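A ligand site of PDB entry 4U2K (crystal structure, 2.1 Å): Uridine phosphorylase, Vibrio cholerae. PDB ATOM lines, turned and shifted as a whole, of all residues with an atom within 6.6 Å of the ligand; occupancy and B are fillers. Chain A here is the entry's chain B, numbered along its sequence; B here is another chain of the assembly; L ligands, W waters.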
ATOM      1  N   ILE A  68      15.463  -6.262  -5.605  1.00  0.00           N
ATOM      2  CA  ILE A  68      15.379  -4.880  -6.093  1.00  0.00           C
ATOM      3  C   ILE A  68      16.042  -3.885  -5.150  1.00  0.00           C
ATOM      4  O   ILE A  68      15.735  -3.837  -3.974  1.00  0.00           O
ATOM      5  CB  ILE A  68      13.922  -4.449  -6.319  1.00  0.00           C
ATOM      6  CG1 ILE A  68      13.227  -5.427  -7.264  1.00  0.00           C
ATOM      7  CG2 ILE A  68      13.863  -3.021  -6.855  1.00  0.00           C
ATOM      8  CD1 ILE A  68      11.793  -5.096  -7.533  1.00  0.00           C
ATOM      9  N   ARG A  90      26.141  -6.926 -14.088  1.00  0.00           N
ATOM     10  CA  ARG A  90      24.728  -6.639 -13.942  1.00  0.00           C
ATOM     11  C   ARG A  90      24.072  -6.779 -15.295  1.00  0.00           C
ATOM     12  O   ARG A  90      24.559  -6.218 -16.275  1.00  0.00           O
ATOM     13  CB  ARG A  90      24.540  -5.229 -13.421  1.00  0.00           C
ATOM     14  CG  ARG A  90      23.099  -4.832 -13.353  1.00  0.00           C
ATOM     15  CD  ARG A  90      22.412  -5.684 -12.369  1.00  0.00           C
ATOM     16  NE  ARG A  90      20.998  -5.372 -12.255  1.00  0.00           N
ATOM     17  CZ  ARG A  90      20.230  -5.852 -11.280  1.00  0.00           C
ATOM     18  NH1 ARG A  90      20.749  -6.649 -10.340  1.00  0.00           N
ATOM     19  NH2 ARG A  90      18.948  -5.527 -11.243  1.00  0.00           N
ATOM     20  N   THR A  93      16.584  -5.037 -17.331  1.00  0.00           N
ATOM     21  CA  THR A  93      15.796  -4.235 -18.255  1.00  0.00           C
ATOM     22  C   THR A  93      15.900  -2.794 -17.819  1.00  0.00           C
ATOM     23  O   THR A  93      16.165  -2.529 -16.647  1.00  0.00           O
ATOM     24  CB  THR A  93      14.314  -4.595 -18.241  1.00  0.00           C
ATOM     25  OG1 THR A  93      13.804  -4.494 -16.896  1.00  0.00           O
ATOM     26  CG2 THR A  93      14.101  -5.996 -18.775  1.00  0.00           C
ATOM     27  N   THR A  94      15.687  -1.877 -18.750  1.00  0.00           N
ATOM     28  CA  THR A  94      15.742  -0.462 -18.391  1.00  0.00           C
ATOM     29  C   THR A  94      14.791   0.367 -19.259  1.00  0.00           C
ATOM     30  O   THR A  94      14.251  -0.113 -20.253  1.00  0.00           O
ATOM     31  CB  THR A  94      17.169   0.102 -18.505  1.00  0.00           C
ATOM     32  OG1 THR A  94      17.183   1.439 -17.999  1.00  0.00           O
ATOM     33  CG2 THR A  94      17.655   0.098 -19.959  1.00  0.00           C
ATOM     34  N   GLY A  95      14.608   1.622 -18.862  1.00  0.00           N
ATOM     35  CA  GLY A  95      13.789   2.546 -19.620  1.00  0.00           C
ATOM     36  C   GLY A  95      14.569   3.785 -20.036  1.00  0.00           C
ATOM     37  O   GLY A  95      15.031   4.562 -19.188  1.00  0.00           O
ATOM     38  N   ALA A  96      14.715   3.976 -21.333  1.00  0.00           N
ATOM     39  CA  ALA A  96      15.501   5.092 -21.856  1.00  0.00           C
ATOM     40  C   ALA A  96      14.738   6.404 -21.685  1.00  0.00           C
ATOM     41  O   ALA A  96      13.529   6.414 -21.525  1.00  0.00           O
ATOM     42  CB  ALA A  96      15.877   4.863 -23.316  1.00  0.00           C
ATOM     43  N   SER A 158      18.321   5.040  -9.371  1.00  0.00           N
ATOM     44  CA  SER A 158      17.359   5.604  -8.428  1.00  0.00           C
ATOM     45  C   SER A 158      16.960   4.585  -7.371  1.00  0.00           C
ATOM     46  O   SER A 158      16.685   3.433  -7.700  1.00  0.00           O
ATOM     47  CB  SER A 158      16.112   6.043  -9.227  1.00  0.00           C
ATOM     48  OG  SER A 158      15.071   6.518  -8.385  1.00  0.00           O
ATOM     49  N   THR A 160      14.195   4.759  -6.061  1.00  0.00           N
ATOM     50  CA  THR A 160      12.740   4.551  -6.213  1.00  0.00           C
ATOM     51  C   THR A 160      12.336   4.305  -7.662  1.00  0.00           C
ATOM     52  O   THR A 160      12.990   4.797  -8.581  1.00  0.00           O
ATOM     53  CB  THR A 160      11.898   5.703  -5.621  1.00  0.00           C
ATOM     54  OG1 THR A 160      12.428   6.972  -6.029  1.00  0.00           O
ATOM     55  CG2 THR A 160      11.884   5.659  -4.130  1.00  0.00           C
ATOM     56  N   PHE A 161      11.289   3.498  -7.850  1.00  0.00           N
ATOM     57  CA  PHE A 161      10.754   3.258  -9.177  1.00  0.00           C
ATOM     58  C   PHE A 161       9.891   4.448  -9.573  1.00  0.00           C
ATOM     59  O   PHE A 161       9.776   4.794 -10.747  1.00  0.00           O
ATOM     60  CB  PHE A 161       9.907   1.977  -9.244  1.00  0.00           C
ATOM     61  CG  PHE A 161       9.390   1.686 -10.643  1.00  0.00           C
ATOM     62  CD1 PHE A 161      10.170   0.990 -11.545  1.00  0.00           C
ATOM     63  CD2 PHE A 161       8.151   2.159 -11.060  1.00  0.00           C
ATOM     64  CE1 PHE A 161       9.723   0.736 -12.832  1.00  0.00           C
ATOM     65  CE2 PHE A 161       7.674   1.909 -12.344  1.00  0.00           C
ATOM     66  CZ  PHE A 161       8.466   1.206 -13.248  1.00  0.00           C
ATOM     67  N   GLN A 165      12.316   8.606 -10.363  1.00  0.00           N
ATOM     68  CA  GLN A 165      12.324   8.618 -11.835  1.00  0.00           C
ATOM     69  C   GLN A 165      11.270   9.587 -12.356  1.00  0.00           C
ATOM     70  O   GLN A 165      10.832   9.525 -13.510  1.00  0.00           O
ATOM     71  CB  GLN A 165      12.113   7.195 -12.386  1.00  0.00           C
ATOM     72  CG  GLN A 165      13.083   6.152 -11.751  1.00  0.00           C
ATOM     73  CD  GLN A 165      12.968   4.748 -12.367  1.00  0.00           C
ATOM     74  OE1 GLN A 165      12.319   4.576 -13.381  1.00  0.00           O
ATOM     75  NE2 GLN A 165      13.592   3.752 -11.732  1.00  0.00           N
ATOM     76  N   ARG A 167       8.020   9.926 -11.928  1.00  0.00           N
ATOM     77  CA  ARG A 167       6.692   9.483 -12.333  1.00  0.00           C
ATOM     78  C   ARG A 167       5.668  10.175 -11.484  1.00  0.00           C
ATOM     79  O   ARG A 167       5.839  10.297 -10.281  1.00  0.00           O
ATOM     80  CB  ARG A 167       6.533   7.964 -12.206  1.00  0.00           C
ATOM     81  CG  ARG A 167       7.315   7.229 -13.269  1.00  0.00           C
ATOM     82  CD  ARG A 167       7.089   5.729 -13.269  1.00  0.00           C
ATOM     83  NE  ARG A 167       7.568   5.188 -14.537  1.00  0.00           N
ATOM     84  CZ  ARG A 167       8.828   4.851 -14.772  1.00  0.00           C
ATOM     85  NH1 ARG A 167       9.739   4.954 -13.808  1.00  0.00           N
ATOM     86  NH2 ARG A 167       9.168   4.379 -15.968  1.00  0.00           N
ATOM     87  N   PHE A 194      16.994   5.223 -16.918  1.00  0.00           N
ATOM     88  CA  PHE A 194      16.750   5.100 -15.496  1.00  0.00           C
ATOM     89  C   PHE A 194      16.856   3.642 -15.083  1.00  0.00           C
ATOM     90  O   PHE A 194      16.340   2.760 -15.773  1.00  0.00           O
ATOM     91  CB  PHE A 194      15.332   5.561 -15.145  1.00  0.00           C
ATOM     92  CG  PHE A 194      15.196   7.034 -14.858  1.00  0.00           C
ATOM     93  CD1 PHE A 194      15.857   7.617 -13.802  1.00  0.00           C
ATOM     94  CD2 PHE A 194      14.320   7.819 -15.625  1.00  0.00           C
ATOM     95  CE1 PHE A 194      15.716   8.992 -13.526  1.00  0.00           C
ATOM     96  CE2 PHE A 194      14.167   9.189 -15.355  1.00  0.00           C
ATOM     97  CZ  PHE A 194      14.857   9.779 -14.294  1.00  0.00           C
ATOM     98  N   GLU A 195      17.505   3.389 -13.950  1.00  0.00           N
ATOM     99  CA  GLU A 195      17.364   2.095 -13.293  1.00  0.00           C
ATOM    100  C   GLU A 195      17.684   2.180 -11.802  1.00  0.00           C
ATOM    101  O   GLU A 195      17.827   3.288 -11.249  1.00  0.00           O
ATOM    102  CB  GLU A 195      18.163   0.994 -14.018  1.00  0.00           C
ATOM    103  CG  GLU A 195      19.623   1.329 -14.190  1.00  0.00           C
ATOM    104  CD  GLU A 195      20.370   1.086 -12.930  1.00  0.00           C
ATOM    105  OE1 GLU A 195      20.759   2.070 -12.259  1.00  0.00           O
ATOM    106  OE2 GLU A 195      20.502  -0.099 -12.584  1.00  0.00           O
ATOM    107  N   MET A 196      17.770   1.036 -11.125  1.00  0.00           N
ATOM    108  CA  MET A 196      17.732   1.097  -9.670  1.00  0.00           C
ATOM    109  C   MET A 196      18.856   0.430  -8.897  1.00  0.00           C
ATOM    110  O   MET A 196      18.793   0.391  -7.678  1.00  0.00           O
ATOM    111  CB  MET A 196      16.394   0.579  -9.160  1.00  0.00           C
ATOM    112  CG  MET A 196      15.179   1.318  -9.730  1.00  0.00           C
ATOM    113  SD  MET A 196      13.685   0.645  -8.991  1.00  0.00           S
ATOM    114  CE  MET A 196      14.289   0.502  -7.297  1.00  0.00           C
ATOM    115  N   GLU A 197      19.875  -0.075  -9.582  1.00  0.00           N
ATOM    116  CA  GLU A 197      20.940  -0.798  -8.894  1.00  0.00           C
ATOM    117  C   GLU A 197      22.349  -0.348  -9.247  1.00  0.00           C
ATOM    118  O   GLU A 197      23.266  -0.577  -8.476  1.00  0.00           O
ATOM    119  CB  GLU A 197      20.818  -2.319  -9.128  1.00  0.00           C
ATOM    120  CG  GLU A 197      19.617  -2.996  -8.449  1.00  0.00           C
ATOM    121  CD  GLU A 197      18.342  -2.769  -9.240  1.00  0.00           C
ATOM    122  OE1 GLU A 197      18.476  -2.575 -10.470  1.00  0.00           O
ATOM    123  OE2 GLU A 197      17.235  -2.790  -8.651  1.00  0.00           O
ATOM    124  N   ILE A 219      13.286  -1.585 -22.752  1.00  0.00           N
ATOM    125  CA  ILE A 219      11.905  -2.096 -22.823  1.00  0.00           C
ATOM    126  C   ILE A 219      10.845  -0.978 -22.869  1.00  0.00           C
ATOM    127  O   ILE A 219       9.652  -1.247 -22.998  1.00  0.00           O
ATOM    128  CB  ILE A 219      11.536  -3.036 -21.632  1.00  0.00           C
ATOM    129  CG1 ILE A 219      11.582  -2.266 -20.303  1.00  0.00           C
ATOM    130  CG2 ILE A 219      12.433  -4.259 -21.615  1.00  0.00           C
ATOM    131  CD1 ILE A 219      11.014  -3.011 -19.084  1.00  0.00           C
ATOM    132  N   ILE A 220      11.283   0.266 -22.719  1.00  0.00           N
ATOM    133  CA  ILE A 220      10.390   1.409 -22.759  1.00  0.00           C
ATOM    134  C   ILE A 220      11.184   2.697 -22.943  1.00  0.00           C
ATOM    135  O   ILE A 220      12.348   2.808 -22.534  1.00  0.00           O
ATOM    136  CB  ILE A 220       9.485   1.485 -21.488  1.00  0.00           C
ATOM    137  CG1 ILE A 220       8.228   2.310 -21.751  1.00  0.00           C
ATOM    138  CG2 ILE A 220      10.258   2.024 -20.290  1.00  0.00           C
ATOM    139  CD1 ILE A 220       7.185   2.229 -20.625  1.00  0.00           C
ATOM    140  N   ARG A 222      10.225   6.720 -22.361  1.00  0.00           N
ATOM    141  CA  ARG A 222       9.176   7.588 -21.834  1.00  0.00           C
ATOM    142  C   ARG A 222       8.926   8.774 -22.761  1.00  0.00           C
ATOM    143  O   ARG A 222       7.925   9.477 -22.600  1.00  0.00           O
ATOM    144  CB  ARG A 222       9.521   8.106 -20.435  1.00  0.00           C
ATOM    145  CG  ARG A 222      10.373   7.182 -19.567  1.00  0.00           C
ATOM    146  CD  ARG A 222       9.634   6.819 -18.296  1.00  0.00           C
ATOM    147  NE  ARG A 222       9.081   7.983 -17.598  1.00  0.00           N
ATOM    148  CZ  ARG A 222       9.556   8.513 -16.477  1.00  0.00           C
ATOM    149  NH1 ARG A 222      10.626   7.985 -15.883  1.00  0.00           N
ATOM    150  NH2 ARG A 222       8.953   9.553 -15.937  1.00  0.00           N
ATOM    151  N   PHE B   6       2.234  -2.758 -11.378  1.00  0.00           N
ATOM    152  CA  PHE B   6       3.315  -3.231 -12.231  1.00  0.00           C
ATOM    153  C   PHE B   6       4.211  -4.344 -11.674  1.00  0.00           C
ATOM    154  O   PHE B   6       4.530  -5.304 -12.382  1.00  0.00           O
ATOM    155  CB  PHE B   6       4.178  -2.055 -12.720  1.00  0.00           C
ATOM    156  CG  PHE B   6       5.261  -2.468 -13.653  1.00  0.00           C
ATOM    157  CD1 PHE B   6       6.575  -2.574 -13.212  1.00  0.00           C
ATOM    158  CD2 PHE B   6       4.975  -2.795 -14.959  1.00  0.00           C
ATOM    159  CE1 PHE B   6       7.582  -2.985 -14.072  1.00  0.00           C
ATOM    160  CE2 PHE B   6       5.968  -3.198 -15.831  1.00  0.00           C
ATOM    161  CZ  PHE B   6       7.274  -3.289 -15.387  1.00  0.00           C
ATOM    162  N   HIS B   7       4.656  -4.223 -10.421  1.00  0.00           N
ATOM    163  CA  HIS B   7       5.475  -5.263  -9.826  1.00  0.00           C
ATOM    164  C   HIS B   7       4.656  -6.318  -9.057  1.00  0.00           C
ATOM    165  O   HIS B   7       5.012  -7.502  -9.071  1.00  0.00           O
ATOM    166  CB  HIS B   7       6.580  -4.658  -8.936  1.00  0.00           C
ATOM    167  CG  HIS B   7       7.452  -3.646  -9.644  1.00  0.00           C
ATOM    168  ND1 HIS B   7       6.973  -2.410 -10.055  1.00  0.00           N
ATOM    169  CD2 HIS B   7       8.743  -3.700  -9.996  1.00  0.00           C
ATOM    170  CE1 HIS B   7       7.970  -1.742 -10.620  1.00  0.00           C
ATOM    171  NE2 HIS B   7       9.047  -2.495 -10.601  1.00  0.00           N
ATOM    172  N   ARG B  47       8.777 -12.150  -8.032  1.00  0.00           N
ATOM    173  CA  ARG B  47       9.995 -11.707  -7.365  1.00  0.00           C
ATOM    174  C   ARG B  47       9.913 -11.875  -5.844  1.00  0.00           C
ATOM    175  O   ARG B  47       9.439 -12.894  -5.351  1.00  0.00           O
ATOM    176  CB  ARG B  47      10.296 -10.243  -7.677  1.00  0.00           C
ATOM    177  CG  ARG B  47      10.587  -9.928  -9.127  1.00  0.00           C
ATOM    178  CD  ARG B  47      10.571  -8.426  -9.330  1.00  0.00           C
ATOM    179  NE  ARG B  47      11.626  -7.921 -10.205  1.00  0.00           N
ATOM    180  CZ  ARG B  47      12.910  -7.847  -9.877  1.00  0.00           C
ATOM    181  NH1 ARG B  47      13.343  -8.282  -8.697  1.00  0.00           N
ATOM    182  NH2 ARG B  47      13.780  -7.358 -10.748  1.00  0.00           N
ATOM    183  N   ILE B  75       8.368   0.344  -3.525  1.00  0.00           N
ATOM    184  CA  ILE B  75       7.569  -0.256  -4.583  1.00  0.00           C
ATOM    185  C   ILE B  75       6.289  -0.962  -4.099  1.00  0.00           C
ATOM    186  O   ILE B  75       5.202  -0.679  -4.603  1.00  0.00           O
ATOM    187  CB  ILE B  75       8.405  -1.235  -5.420  1.00  0.00           C
ATOM    188  CG1 ILE B  75       9.413  -0.458  -6.261  1.00  0.00           C
ATOM    189  CG2 ILE B  75       7.497  -2.080  -6.314  1.00  0.00           C
ATOM    190  CD1 ILE B  75      10.464  -1.323  -6.888  1.00  0.00           C
HETATM  191  C1  LIG L   1      13.496   1.115 -13.926  1.00  0.00           C
HETATM  192  C2  LIG L   1      12.346   2.117 -15.684  1.00  0.00           C
HETATM  193  C3  LIG L   1      12.232   0.886 -16.354  1.00  0.00           C
HETATM  194  F1  LIG L   1      11.587   0.890 -17.557  1.00  0.00           F
HETATM  195  C4  LIG L   1      12.777  -0.224 -15.787  1.00  0.00           C
HETATM  196  O1  LIG L   1      14.053   1.253 -12.827  1.00  0.00           O
HETATM  197  N1  LIG L   1      12.981   2.175 -14.495  1.00  0.00           N
HETATM  198  O2  LIG L   1      11.828   3.222 -16.219  1.00  0.00           O
HETATM  199  N2  LIG L   1      13.418  -0.092 -14.554  1.00  0.00           N
HETATM  200  C5  LIG L   1      14.003  -1.229 -13.852  1.00  0.00           C
HETATM  201  C6  LIG L   1      13.276  -1.487 -12.542  1.00  0.00           C
HETATM  202  N3  LIG L   1      13.933  -2.378 -11.642  1.00  0.00           N
HETATM  203  C7  LIG L   1      11.821  -1.897 -12.745  1.00  0.00           C
HETATM  204  N4  LIG L   1      11.494  -3.264 -12.505  1.00  0.00           N
HETATM  205  O   HOH W   1      16.901  -1.916 -12.212  1.00  0.00           O
HETATM  206  O   HOH W   2      10.763  -6.240 -11.828  1.00  0.00           O
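OE1 of Gln 165 sits at hydrogen-bond distance from N1 of the ligand.
An oxygen (O2) of the ligand lies within hydrogen-bond range of the guanidinium group (NH2) of Arg 167, 2.9 Å away.
A ring nitrogen (NE2) of His 7 of chain B sits at hydrogen-bond distance from a nitrogen (N4) of the ligand, at 3.2 Å.
OE1 of Gln 165 sits at hydrogen-bond distance from NH1 of Arg 167 (2.6 Å).
The backbone carbonyl oxygen of Gln 165 lies within hydrogen-bond range of the guanidinium group of Arg 222 (2.8 Å).
The backbone carbonyl oxygen of Thr 160 lies within hydrogen-bond range of the side-chain amide nitrogen of Gln 165, 3.4 Å away.
NH1 of Arg 167 lies within hydrogen-bond range of O of Phe 161.
O of Ile 220 lies within hydrogen-bond range of N of Ala 96 (2.9 Å).
OE2 of Glu 195 is in hydrogen-bond range of N of Glu 197 (3.1 Å).
O of Phe 194 lies within hydrogen-bond range of OG1 of Thr 94 (2.7 Å).
O of Thr 94 sits at hydrogen-bond distance from N of Ile 219 (3.1 Å).
N of Gly 95 lies close to F1 of the ligand (3.4 Å).
Merely in contact with the ligand: Ile 220 (3.2 Å), Met 196 (3.3 Å), Phe 161 (3.4 Å), Glu 195 (3.4 Å), Phe 194 (3.6 Å), Thr 94 (3.7 Å) and Thr 93 (3.8 Å).
Hydrophobic or aromatic side chains within 4 Å of the ligand: Phe 161, Met 196, Ile 220 and His 7 of chain B.
Water W1 lies within hydrogen-bond range of the side-chain carboxylate (OE1) of Glu 197 (2.4 Å), a nitrogen (N3) of the ligand (3.1 Å) and the backbone NH (N) of Met 196 (3.3 Å).
Water W2 lies within hydrogen-bond range of the guanidinium group of Arg 47 of chain B (2.5 Å) and a nitrogen (N4) of the ligand (3.1 Å).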
